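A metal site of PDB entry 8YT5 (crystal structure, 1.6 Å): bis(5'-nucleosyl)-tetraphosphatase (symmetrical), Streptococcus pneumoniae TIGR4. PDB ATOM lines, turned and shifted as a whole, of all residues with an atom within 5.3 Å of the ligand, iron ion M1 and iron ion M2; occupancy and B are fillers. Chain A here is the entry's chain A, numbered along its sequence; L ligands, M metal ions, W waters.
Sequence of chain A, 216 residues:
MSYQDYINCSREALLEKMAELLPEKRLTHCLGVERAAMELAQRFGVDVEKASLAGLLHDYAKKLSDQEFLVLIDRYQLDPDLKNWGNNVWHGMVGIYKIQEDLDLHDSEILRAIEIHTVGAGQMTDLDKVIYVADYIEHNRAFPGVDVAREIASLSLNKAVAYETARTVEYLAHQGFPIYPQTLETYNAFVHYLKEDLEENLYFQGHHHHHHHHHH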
ATOM      1  N   ARG A  26      42.031 -19.823   2.635  1.00  0.00           N
ATOM      2  CA  ARG A  26      41.255 -18.792   3.317  1.00  0.00           C
ATOM      3  C   ARG A  26      42.143 -17.632   3.770  1.00  0.00           C
ATOM      4  O   ARG A  26      41.728 -16.467   3.668  1.00  0.00           O
ATOM      5  CB  ARG A  26      40.475 -19.408   4.488  1.00  0.00           C
ATOM      6  CG  ARG A  26      39.459 -18.476   5.171  1.00  0.00           C
ATOM      7  CD  ARG A  26      38.432 -17.861   4.230  1.00  0.00           C
ATOM      8  NE  ARG A  26      37.678 -18.864   3.484  1.00  0.00           N
ATOM      9  CZ  ARG A  26      36.696 -18.591   2.631  1.00  0.00           C
ATOM     10  NH1 ARG A  26      36.313 -17.336   2.409  1.00  0.00           N
ATOM     11  NH2 ARG A  26      36.087 -19.584   1.989  1.00  0.00           N
ATOM     12  N   HIS A  29      42.986 -15.638   0.790  1.00  0.00           N
ATOM     13  CA  HIS A  29      41.828 -14.790   0.488  1.00  0.00           C
ATOM     14  C   HIS A  29      41.829 -13.535   1.366  1.00  0.00           C
ATOM     15  O   HIS A  29      41.620 -12.435   0.876  1.00  0.00           O
ATOM     16  CB  HIS A  29      40.531 -15.584   0.604  1.00  0.00           C
ATOM     17  CG  HIS A  29      39.299 -14.744   0.754  1.00  0.00           C
ATOM     18  ND1 HIS A  29      38.756 -14.024  -0.285  1.00  0.00           N
ATOM     19  CD2 HIS A  29      38.483 -14.522   1.822  1.00  0.00           C
ATOM     20  CE1 HIS A  29      37.671 -13.388   0.135  1.00  0.00           C
ATOM     21  NE2 HIS A  29      37.481 -13.682   1.403  1.00  0.00           N
ATOM     22  N   VAL A  33      41.905  -9.636   0.293  1.00  0.00           N
ATOM     23  CA  VAL A  33      40.925  -8.638   0.728  1.00  0.00           C
ATOM     24  C   VAL A  33      41.630  -7.436   1.388  1.00  0.00           C
ATOM     25  O   VAL A  33      41.237  -6.287   1.173  1.00  0.00           O
ATOM     26  CB  VAL A  33      39.829  -9.261   1.615  1.00  0.00           C
ATOM     27  CG1 VAL A  33      38.808  -8.227   2.039  1.00  0.00           C
ATOM     28  CG2 VAL A  33      39.115 -10.389   0.882  1.00  0.00           C
ATOM     29  N   HIS A  58      38.295  -9.914   8.025  1.00  0.00           N
ATOM     30  CA  HIS A  58      36.851 -10.079   7.789  1.00  0.00           C
ATOM     31  C   HIS A  58      36.396 -11.541   7.911  1.00  0.00           C
ATOM     32  O   HIS A  58      35.292 -11.800   8.378  1.00  0.00           O
ATOM     33  CB  HIS A  58      36.438  -9.482   6.449  1.00  0.00           C
ATOM     34  CG  HIS A  58      36.703 -10.376   5.291  1.00  0.00           C
ATOM     35  ND1 HIS A  58      37.972 -10.629   4.839  1.00  0.00           N
ATOM     36  CD2 HIS A  58      35.872 -11.143   4.549  1.00  0.00           C
ATOM     37  CE1 HIS A  58      37.919 -11.482   3.832  1.00  0.00           C
ATOM     38  NE2 HIS A  58      36.649 -11.820   3.641  1.00  0.00           N
ATOM     39  N   ASP A  59      37.254 -12.489   7.509  1.00  0.00           N
ATOM     40  CA  ASP A  59      36.932 -13.915   7.601  1.00  0.00           C
ATOM     41  C   ASP A  59      37.681 -14.634   8.715  1.00  0.00           C
ATOM     42  O   ASP A  59      37.802 -15.856   8.683  1.00  0.00           O
ATOM     43  CB  ASP A  59      37.154 -14.628   6.251  1.00  0.00           C
ATOM     44  CG  ASP A  59      35.963 -14.493   5.299  1.00  0.00           C
ATOM     45  OD1 ASP A  59      34.832 -14.202   5.735  1.00  0.00           O
ATOM     46  OD2 ASP A  59      36.168 -14.673   4.083  1.00  0.00           O
ATOM     47  N   LYS A  62      35.772 -17.604  10.161  1.00  0.00           N
ATOM     48  CA  LYS A  62      35.160 -18.496   9.169  1.00  0.00           C
ATOM     49  C   LYS A  62      35.094 -19.962   9.609  1.00  0.00           C
ATOM     50  O   LYS A  62      34.185 -20.687   9.203  1.00  0.00           O
ATOM     51  CB  LYS A  62      35.898 -18.384   7.838  1.00  0.00           C
ATOM     52  CG  LYS A  62      35.251 -19.111   6.653  1.00  0.00           C
ATOM     53  CD  LYS A  62      34.033 -18.395   6.091  1.00  0.00           C
ATOM     54  CE  LYS A  62      33.609 -19.017   4.767  1.00  0.00           C
ATOM     55  NZ  LYS A  62      32.573 -18.205   4.052  1.00  0.00           N
ATOM     56  N   TRP A  85      20.003 -19.846  11.489  1.00  0.00           N
ATOM     57  CA  TRP A  85      20.856 -19.732  10.312  1.00  0.00           C
ATOM     58  C   TRP A  85      22.135 -20.531  10.526  1.00  0.00           C
ATOM     59  O   TRP A  85      22.121 -21.555  11.205  1.00  0.00           O
ATOM     60  CB  TRP A  85      21.089 -18.252   9.983  1.00  0.00           C
ATOM     61  CG  TRP A  85      19.783 -17.567   9.760  1.00  0.00           C
ATOM     62  CD1 TRP A  85      18.985 -16.984  10.701  1.00  0.00           C
ATOM     63  CD2 TRP A  85      19.085 -17.441   8.506  1.00  0.00           C
ATOM     64  NE1 TRP A  85      17.844 -16.483  10.125  1.00  0.00           N
ATOM     65  CE2 TRP A  85      17.871 -16.755   8.779  1.00  0.00           C
ATOM     66  CE3 TRP A  85      19.377 -17.828   7.195  1.00  0.00           C
ATOM     67  CZ2 TRP A  85      16.944 -16.443   7.780  1.00  0.00           C
ATOM     68  CZ3 TRP A  85      18.446 -17.525   6.198  1.00  0.00           C
ATOM     69  CH2 TRP A  85      17.246 -16.840   6.489  1.00  0.00           C
ATOM     70  N   ASN A  88      27.392 -18.973   7.219  1.00  0.00           N
ATOM     71  CA  ASN A  88      27.334 -17.855   6.270  1.00  0.00           C
ATOM     72  C   ASN A  88      26.937 -16.540   6.941  1.00  0.00           C
ATOM     73  O   ASN A  88      27.617 -15.532   6.774  1.00  0.00           O
ATOM     74  CB  ASN A  88      26.378 -18.145   5.101  1.00  0.00           C
ATOM     75  CG  ASN A  88      26.896 -19.249   4.189  1.00  0.00           C
ATOM     76  OD1 ASN A  88      28.036 -19.703   4.298  1.00  0.00           O
ATOM     77  ND2 ASN A  88      26.035 -19.683   3.265  1.00  0.00           N
ATOM     78  N   VAL A  89      25.874 -16.578   7.725  1.00  0.00           N
ATOM     79  CA  VAL A  89      25.428 -15.419   8.491  1.00  0.00           C
ATOM     80  C   VAL A  89      26.341 -15.183   9.689  1.00  0.00           C
ATOM     81  O   VAL A  89      26.741 -14.050   9.970  1.00  0.00           O
ATOM     82  CB  VAL A  89      23.949 -15.593   8.936  1.00  0.00           C
ATOM     83  CG1 VAL A  89      23.520 -14.459   9.850  1.00  0.00           C
ATOM     84  CG2 VAL A  89      23.023 -15.637   7.731  1.00  0.00           C
ATOM     85  N   HIS A  91      29.549 -15.947  10.601  1.00  0.00           N
ATOM     86  CA  HIS A  91      31.005 -15.718  10.719  1.00  0.00           C
ATOM     87  C   HIS A  91      31.347 -14.243  10.766  1.00  0.00           C
ATOM     88  O   HIS A  91      32.302 -13.841  11.417  1.00  0.00           O
ATOM     89  CB  HIS A  91      31.833 -16.493   9.689  1.00  0.00           C
ATOM     90  CG  HIS A  91      31.749 -15.961   8.294  1.00  0.00           C
ATOM     91  ND1 HIS A  91      30.643 -16.146   7.496  1.00  0.00           N
ATOM     92  CD2 HIS A  91      32.632 -15.252   7.560  1.00  0.00           C
ATOM     93  CE1 HIS A  91      30.846 -15.564   6.330  1.00  0.00           C
ATOM     94  NE2 HIS A  91      32.052 -15.024   6.335  1.00  0.00           N
ATOM     95  N   HIS A 117      29.863  -7.788   6.501  1.00  0.00           N
ATOM     96  CA  HIS A 117      30.593  -7.991   5.236  1.00  0.00           C
ATOM     97  C   HIS A 117      29.926  -8.999   4.306  1.00  0.00           C
ATOM     98  O   HIS A 117      30.160  -8.965   3.102  1.00  0.00           O
ATOM     99  CB  HIS A 117      32.054  -8.367   5.482  1.00  0.00           C
ATOM    100  CG  HIS A 117      32.256  -9.833   5.755  1.00  0.00           C
ATOM    101  ND1 HIS A 117      32.307 -10.339   7.031  1.00  0.00           N
ATOM    102  CD2 HIS A 117      32.421 -10.881   4.915  1.00  0.00           C
ATOM    103  CE1 HIS A 117      32.489 -11.649   6.969  1.00  0.00           C
ATOM    104  NE2 HIS A 117      32.567 -12.000   5.704  1.00  0.00           N
ATOM    105  N   THR A 118      29.104  -9.893   4.855  1.00  0.00           N
ATOM    106  CA  THR A 118      28.419 -10.897   4.045  1.00  0.00           C
ATOM    107  C   THR A 118      27.053 -10.401   3.599  1.00  0.00           C
ATOM    108  O   THR A 118      26.718 -10.491   2.406  1.00  0.00           O
ATOM    109  CB  THR A 118      28.220 -12.206   4.829  1.00  0.00           C
ATOM    110  OG1 THR A 118      29.465 -12.660   5.369  1.00  0.00           O
ATOM    111  CG2 THR A 118      27.586 -13.294   3.949  1.00  0.00           C
ATOM    112  N   VAL A 119      26.272  -9.861   4.530  1.00  0.00           N
ATOM    113  CA  VAL A 119      24.875  -9.539   4.265  1.00  0.00           C
ATOM    114  C   VAL A 119      24.601  -8.068   3.935  1.00  0.00           C
ATOM    115  O   VAL A 119      23.514  -7.732   3.455  1.00  0.00           O
ATOM    116  CB  VAL A 119      23.958 -10.012   5.419  1.00  0.00           C
ATOM    117  CG1 VAL A 119      23.976 -11.527   5.507  1.00  0.00           C
ATOM    118  CG2 VAL A 119      24.349  -9.375   6.746  1.00  0.00           C
ATOM    119  N   ASP A 135      35.920  -7.993  -0.566  1.00  0.00           N
ATOM    120  CA  ASP A 135      35.727  -9.424  -0.370  1.00  0.00           C
ATOM    121  C   ASP A 135      35.399 -10.120  -1.692  1.00  0.00           C
ATOM    122  O   ASP A 135      35.878 -11.223  -1.976  1.00  0.00           O
ATOM    123  CB  ASP A 135      34.591  -9.605   0.646  1.00  0.00           C
ATOM    124  CG  ASP A 135      34.358 -11.033   1.046  1.00  0.00           C
ATOM    125  OD1 ASP A 135      35.293 -11.875   1.051  1.00  0.00           O
ATOM    126  OD2 ASP A 135      33.213 -11.308   1.431  1.00  0.00           O
ATOM    127  N   ARG A 141      39.923 -14.272  -6.337  1.00  0.00           N
ATOM    128  CA  ARG A 141      38.576 -14.679  -6.788  1.00  0.00           C
ATOM    129  C   ARG A 141      38.564 -14.930  -8.288  1.00  0.00           C
ATOM    130  O   ARG A 141      39.167 -14.189  -9.050  1.00  0.00           O
ATOM    131  CB  ARG A 141      37.543 -13.600  -6.471  1.00  0.00           C
ATOM    132  CG  ARG A 141      37.374 -13.193  -5.010  1.00  0.00           C
ATOM    133  CD  ARG A 141      37.037 -14.358  -4.114  1.00  0.00           C
ATOM    134  NE  ARG A 141      35.738 -14.957  -4.366  1.00  0.00           N
ATOM    135  CZ  ARG A 141      34.610 -14.573  -3.783  1.00  0.00           C
ATOM    136  NH1 ARG A 141      34.623 -13.562  -2.921  1.00  0.00           N
ATOM    137  NH2 ARG A 141      33.477 -15.195  -4.026  1.00  0.00           N
ATOM    138  N   GLU A 164      27.072  -6.631  -6.653  1.00  0.00           N
ATOM    139  CA  GLU A 164      27.384  -7.800  -5.831  1.00  0.00           C
ATOM    140  C   GLU A 164      26.118  -8.355  -5.175  1.00  0.00           C
ATOM    141  O   GLU A 164      25.901  -9.568  -5.167  1.00  0.00           O
ATOM    142  CB  GLU A 164      28.431  -7.476  -4.767  1.00  0.00           C
ATOM    143  CG  GLU A 164      28.724  -8.676  -3.881  1.00  0.00           C
ATOM    144  CD  GLU A 164      29.733  -8.396  -2.791  1.00  0.00           C
ATOM    145  OE1 GLU A 164      30.402  -7.344  -2.852  1.00  0.00           O
ATOM    146  OE2 GLU A 164      29.869  -9.247  -1.890  1.00  0.00           O
ATOM    147  N   THR A 168      24.334 -11.970  -5.748  1.00  0.00           N
ATOM    148  CA  THR A 168      24.224 -12.868  -4.614  1.00  0.00           C
ATOM    149  C   THR A 168      22.790 -13.352  -4.389  1.00  0.00           C
ATOM    150  O   THR A 168      22.564 -14.548  -4.205  1.00  0.00           O
ATOM    151  CB  THR A 168      24.811 -12.221  -3.361  1.00  0.00           C
ATOM    152  OG1 THR A 168      26.223 -12.082  -3.573  1.00  0.00           O
ATOM    153  CG2 THR A 168      24.584 -13.101  -2.133  1.00  0.00           C
ATOM    154  N   LEU A 172      21.691 -17.219  -4.818  1.00  0.00           N
ATOM    155  CA  LEU A 172      21.081 -17.972  -3.726  1.00  0.00           C
ATOM    156  C   LEU A 172      19.746 -18.559  -4.164  1.00  0.00           C
ATOM    157  O   LEU A 172      19.464 -19.730  -3.886  1.00  0.00           O
ATOM    158  CB  LEU A 172      20.927 -17.104  -2.486  1.00  0.00           C
ATOM    159  CG  LEU A 172      22.235 -16.702  -1.815  1.00  0.00           C
ATOM    160  CD1 LEU A 172      21.993 -15.601  -0.808  1.00  0.00           C
ATOM    161  CD2 LEU A 172      22.933 -17.892  -1.171  1.00  0.00           C
ATOM    162  N   PRO A 178      18.181 -20.605   1.522  1.00  0.00           N
ATOM    163  CA  PRO A 178      17.521 -19.521   2.254  1.00  0.00           C
ATOM    164  C   PRO A 178      18.334 -18.231   2.183  1.00  0.00           C
ATOM    165  O   PRO A 178      19.580 -18.267   2.142  1.00  0.00           O
ATOM    166  CB  PRO A 178      17.477 -20.043   3.695  1.00  0.00           C
ATOM    167  CG  PRO A 178      17.605 -21.524   3.580  1.00  0.00           C
ATOM    168  CD  PRO A 178      18.505 -21.741   2.405  1.00  0.00           C
ATOM    169  N   ILE A 179      17.636 -17.101   2.129  1.00  0.00           N
ATOM    170  CA  ILE A 179      18.275 -15.798   2.038  1.00  0.00           C
ATOM    171  C   ILE A 179      18.020 -15.031   3.326  1.00  0.00           C
ATOM    172  O   ILE A 179      16.877 -14.709   3.649  1.00  0.00           O
ATOM    173  CB  ILE A 179      17.760 -15.005   0.814  1.00  0.00           C
ATOM    174  CG1 ILE A 179      18.105 -15.755  -0.479  1.00  0.00           C
ATOM    175  CG2 ILE A 179      18.332 -13.588   0.797  1.00  0.00           C
ATOM    176  CD1 ILE A 179      17.313 -15.300  -1.695  1.00  0.00           C
ATOM    177  N   TYR A 180      19.096 -14.750   4.058  1.00  0.00           N
ATOM    178  CA  TYR A 180      18.975 -13.967   5.280  1.00  0.00           C
ATOM    179  C   TYR A 180      18.351 -12.617   4.948  1.00  0.00           C
ATOM    180  O   TYR A 180      18.797 -11.951   4.024  1.00  0.00           O
ATOM    181  CB  TYR A 180      20.342 -13.775   5.927  1.00  0.00           C
ATOM    182  CG  TYR A 180      20.276 -13.198   7.309  1.00  0.00           C
ATOM    183  CD1 TYR A 180      19.728 -13.932   8.361  1.00  0.00           C
ATOM    184  CD2 TYR A 180      20.762 -11.917   7.573  1.00  0.00           C
ATOM    185  CE1 TYR A 180      19.656 -13.400   9.644  1.00  0.00           C
ATOM    186  CE2 TYR A 180      20.702 -11.379   8.858  1.00  0.00           C
ATOM    187  CZ  TYR A 180      20.153 -12.131   9.882  1.00  0.00           C
ATOM    188  OH  TYR A 180      20.085 -11.603  11.156  1.00  0.00           O
ATOM    189  N   THR A 183      20.069  -9.223   3.833  1.00  0.00           N
ATOM    190  CA  THR A 183      20.525  -9.128   2.449  1.00  0.00           C
ATOM    191  C   THR A 183      19.515  -8.460   1.528  1.00  0.00           C
ATOM    192  O   THR A 183      19.876  -7.693   0.640  1.00  0.00           O
ATOM    193  CB  THR A 183      20.941 -10.514   1.922  1.00  0.00           C
ATOM    194  OG1 THR A 183      22.091 -10.928   2.675  1.00  0.00           O
ATOM    195  CG2 THR A 183      21.273 -10.504   0.442  1.00  0.00           C
HETATM  196  P1  LIG L   1      33.382 -15.519   1.960  1.00  0.00           P
HETATM  197  O1  LIG L   1      33.114 -16.851   1.295  1.00  0.00           O
HETATM  198  O2  LIG L   1      34.690 -14.917   1.512  1.00  0.00           O
HETATM  199  O3  LIG L   1      33.278 -15.559   3.481  1.00  0.00           O
HETATM  200  P2  LIG L   1      30.879 -14.017   2.113  1.00  0.00           P
HETATM  201  O4  LIG L   1      30.365 -12.773   1.418  1.00  0.00           O
HETATM  202  O5  LIG L   1      31.048 -13.903   3.599  1.00  0.00           O
HETATM  203  O6  LIG L   1      32.266 -14.476   1.403  1.00  0.00           O
HETATM  204  O7  LIG L   1      29.795 -15.154   1.813  1.00  0.00           O
HETATM  205  C1  LIG L   1      29.962 -16.487   2.283  1.00  0.00           C
HETATM  206  C2  LIG L   1      28.756 -17.304   1.814  1.00  0.00           C
HETATM  207  O8  LIG L   1      27.549 -16.729   2.361  1.00  0.00           O
HETATM  208  C3  LIG L   1      28.642 -17.359   0.301  1.00  0.00           C
HETATM  209  O9  LIG L   1      28.431 -18.726  -0.101  1.00  0.00           O
HETATM  210  C4  LIG L   1      27.391 -16.538   0.089  1.00  0.00           C
HETATM  211  O10 LIG L   1      26.664 -17.040  -1.006  1.00  0.00           O
HETATM  212  C5  LIG L   1      26.578 -16.758   1.353  1.00  0.00           C
HETATM  213  N1  LIG L   1      25.553 -15.739   1.583  1.00  0.00           N
HETATM  214  C6  LIG L   1      25.641 -14.445   1.251  1.00  0.00           C
HETATM  215  N2  LIG L   1      24.506 -13.808   1.591  1.00  0.00           N
HETATM  216  C7  LIG L   1      23.692 -14.705   2.144  1.00  0.00           C
HETATM  217  C8  LIG L   1      22.341 -14.700   2.705  1.00  0.00           C
HETATM  218  N3  LIG L   1      21.601 -13.579   2.766  1.00  0.00           N
HETATM  219  N4  LIG L   1      21.854 -15.858   3.172  1.00  0.00           N
HETATM  220  C9  LIG L   1      22.553 -17.003   3.129  1.00  0.00           C
HETATM  221  N5  LIG L   1      23.792 -17.077   2.631  1.00  0.00           N
HETATM  222  C10 LIG L   1      24.388 -15.974   2.130  1.00  0.00           C
HETATM  223 FE    FE M   1      35.649 -13.308   2.430  1.00  0.00          FE
HETATM  224 FE    FE M   2      32.996 -13.959   4.708  1.00  0.00          FE
HETATM  225  O   HOH W   1      31.980 -19.696   1.175  1.00  0.00           O
HETATM  226  O   HOH W   2      24.498 -11.118   1.014  1.00  0.00           O
HETATM  227  O   HOH W   3      34.137 -18.609  -0.404  1.00  0.00           O
HETATM  228  O   HOH W   4      23.849 -20.404   1.611  1.00  0.00           O
HETATM  229  O   HOH W   5      30.783  -9.952   0.624  1.00  0.00           O
HETATM  230  O   HOH W   6      31.939 -16.449  -1.220  1.00  0.00           O
HETATM  231  O   HOH W   7      35.801 -16.042  -1.179  1.00  0.00           O
HETATM  232  O   HOH W   8      25.782 -20.185  -0.325  1.00  0.00           O
HETATM  233  O   HOH W   9      33.929 -12.999   3.264  1.00  0.00           O
HETATM  234  O   HOH W  10      21.481 -20.028   3.019  1.00  0.00           O
HETATM  235  O   HOH W  11      32.143 -12.362  -1.231  1.00  0.00           O
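A ring nitrogen (NE2) of His 117 lies close to the side-chain hydroxyl (OG1) of Thr 118, 3.2 Å away.
OD2 of Asp 59 lies close to NH1 of Arg 26.
The backbone carbonyl oxygen (O) of Asn 88 sits at hydrogen-bond distance from a ring nitrogen (ND1) of His 91 (3.2 Å).
O of Asp 135 sits at hydrogen-bond distance from NH1 of Arg 141, 2.8 Å away.
The side-chain hydroxyl (OG1) of Thr 168 is in hydrogen-bond range of the backbone carbonyl oxygen (O) of Glu 164 (3.0 Å).
An oxygen (O8) of the ligand lies close to the side-chain amide nitrogen (ND2) of Asn 88.
The side-chain hydroxyl (OG1) of Thr 118 sits close to an oxygen (O5) of the ligand (2.7 Å).
O1 of the ligand lies within salt-bridge range of NZ of Lys 62, at 3.1 Å.
NH1 of Arg 26 lies within salt-bridge range of O1 of the ligand (3.4 Å).
N of Tyr 180 is in hydrogen-bond range of N4 of the ligand (3.1 Å).
A nitrogen (N3) of the ligand sits at hydrogen-bond distance from the side-chain hydroxyl of Thr 183 (2.7 Å).
A nitrogen (N3) of the ligand sits close to the backbone carbonyl oxygen (O) of Tyr 180 (3.5 Å).
Iron ion M2 is bound by water W9 (2.0 Å), an oxygen (O3) of the ligand (2.0 Å), the side-chain carboxylate (OD1) of Asp 59 (2.1 Å), a ring nitrogen (NE2) of His 91 (2.2 Å), a ring nitrogen (NE2) of His 117 (2.2 Å) and an oxygen (O5) of the ligand (2.2 Å).
Iron ion M2 has six donor atoms within binding distance.
Thr 118 touches iron ion M2 (OG1 to FE, 3.8 Å).
Of the 22 residues printed, 4 come within 4 Å of iron ion M2.
The nearest printed residue that does not touch iron ion M2 is His 58 (4.03 Å).
N4 of the ligand sits close to O of Pro 178 (3.5 Å).
Residues that only touch the ligand: Thr 168 (3.8 Å), Leu 172 (3.5 Å) and Ile 179 (3.8 Å).
Along chain A the residues within 4 Å of the ligand span positions 26 to 183.
Water W9 lies within hydrogen-bond range of OD2 of Asp 135 (2.6 Å) and O6 of the ligand (2.9 Å).
Water W2 lies within hydrogen-bond range of the backbone carbonyl oxygen (O) of Thr 118, a nitrogen (N2) of the ligand and the side-chain hydroxyl (OG1) of Thr 183.
Water W6 bridges an oxygen (O1) of the ligand (2.8 Å) and the guanidinium group of Arg 141 (3.4 Å).
Water W1 bridges an oxygen (O1) of the ligand (3.1 Å) and the side-chain amino group of Lys 62 (3.3 Å).
Water W11 lies within hydrogen-bond range of the side-chain carboxylate (OD2) of Asp 135 (3.1 Å), an oxygen (O4) of the ligand (3.2 Å) and the guanidinium group (NH1) of Arg 141 (3.2 Å).
Water W4 bridges the side-chain amide nitrogen of Asn 88 (2.8 Å) and a nitrogen (N5) of the ligand (3.5 Å).
Four residues have an atom within 4 Å of iron ion M1: His 29, His 58, Asp 59 and Asp 135.
Iron ion M1 is bound by water W9 (1.9 Å), OD1 of Asp 135 (2.0 Å), O2 of the ligand (2.1 Å), NE2 of His 29 (2.1 Å), NE2 of His 58 (2.2 Å) and OD2 of Asp 59 (2.2 Å).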
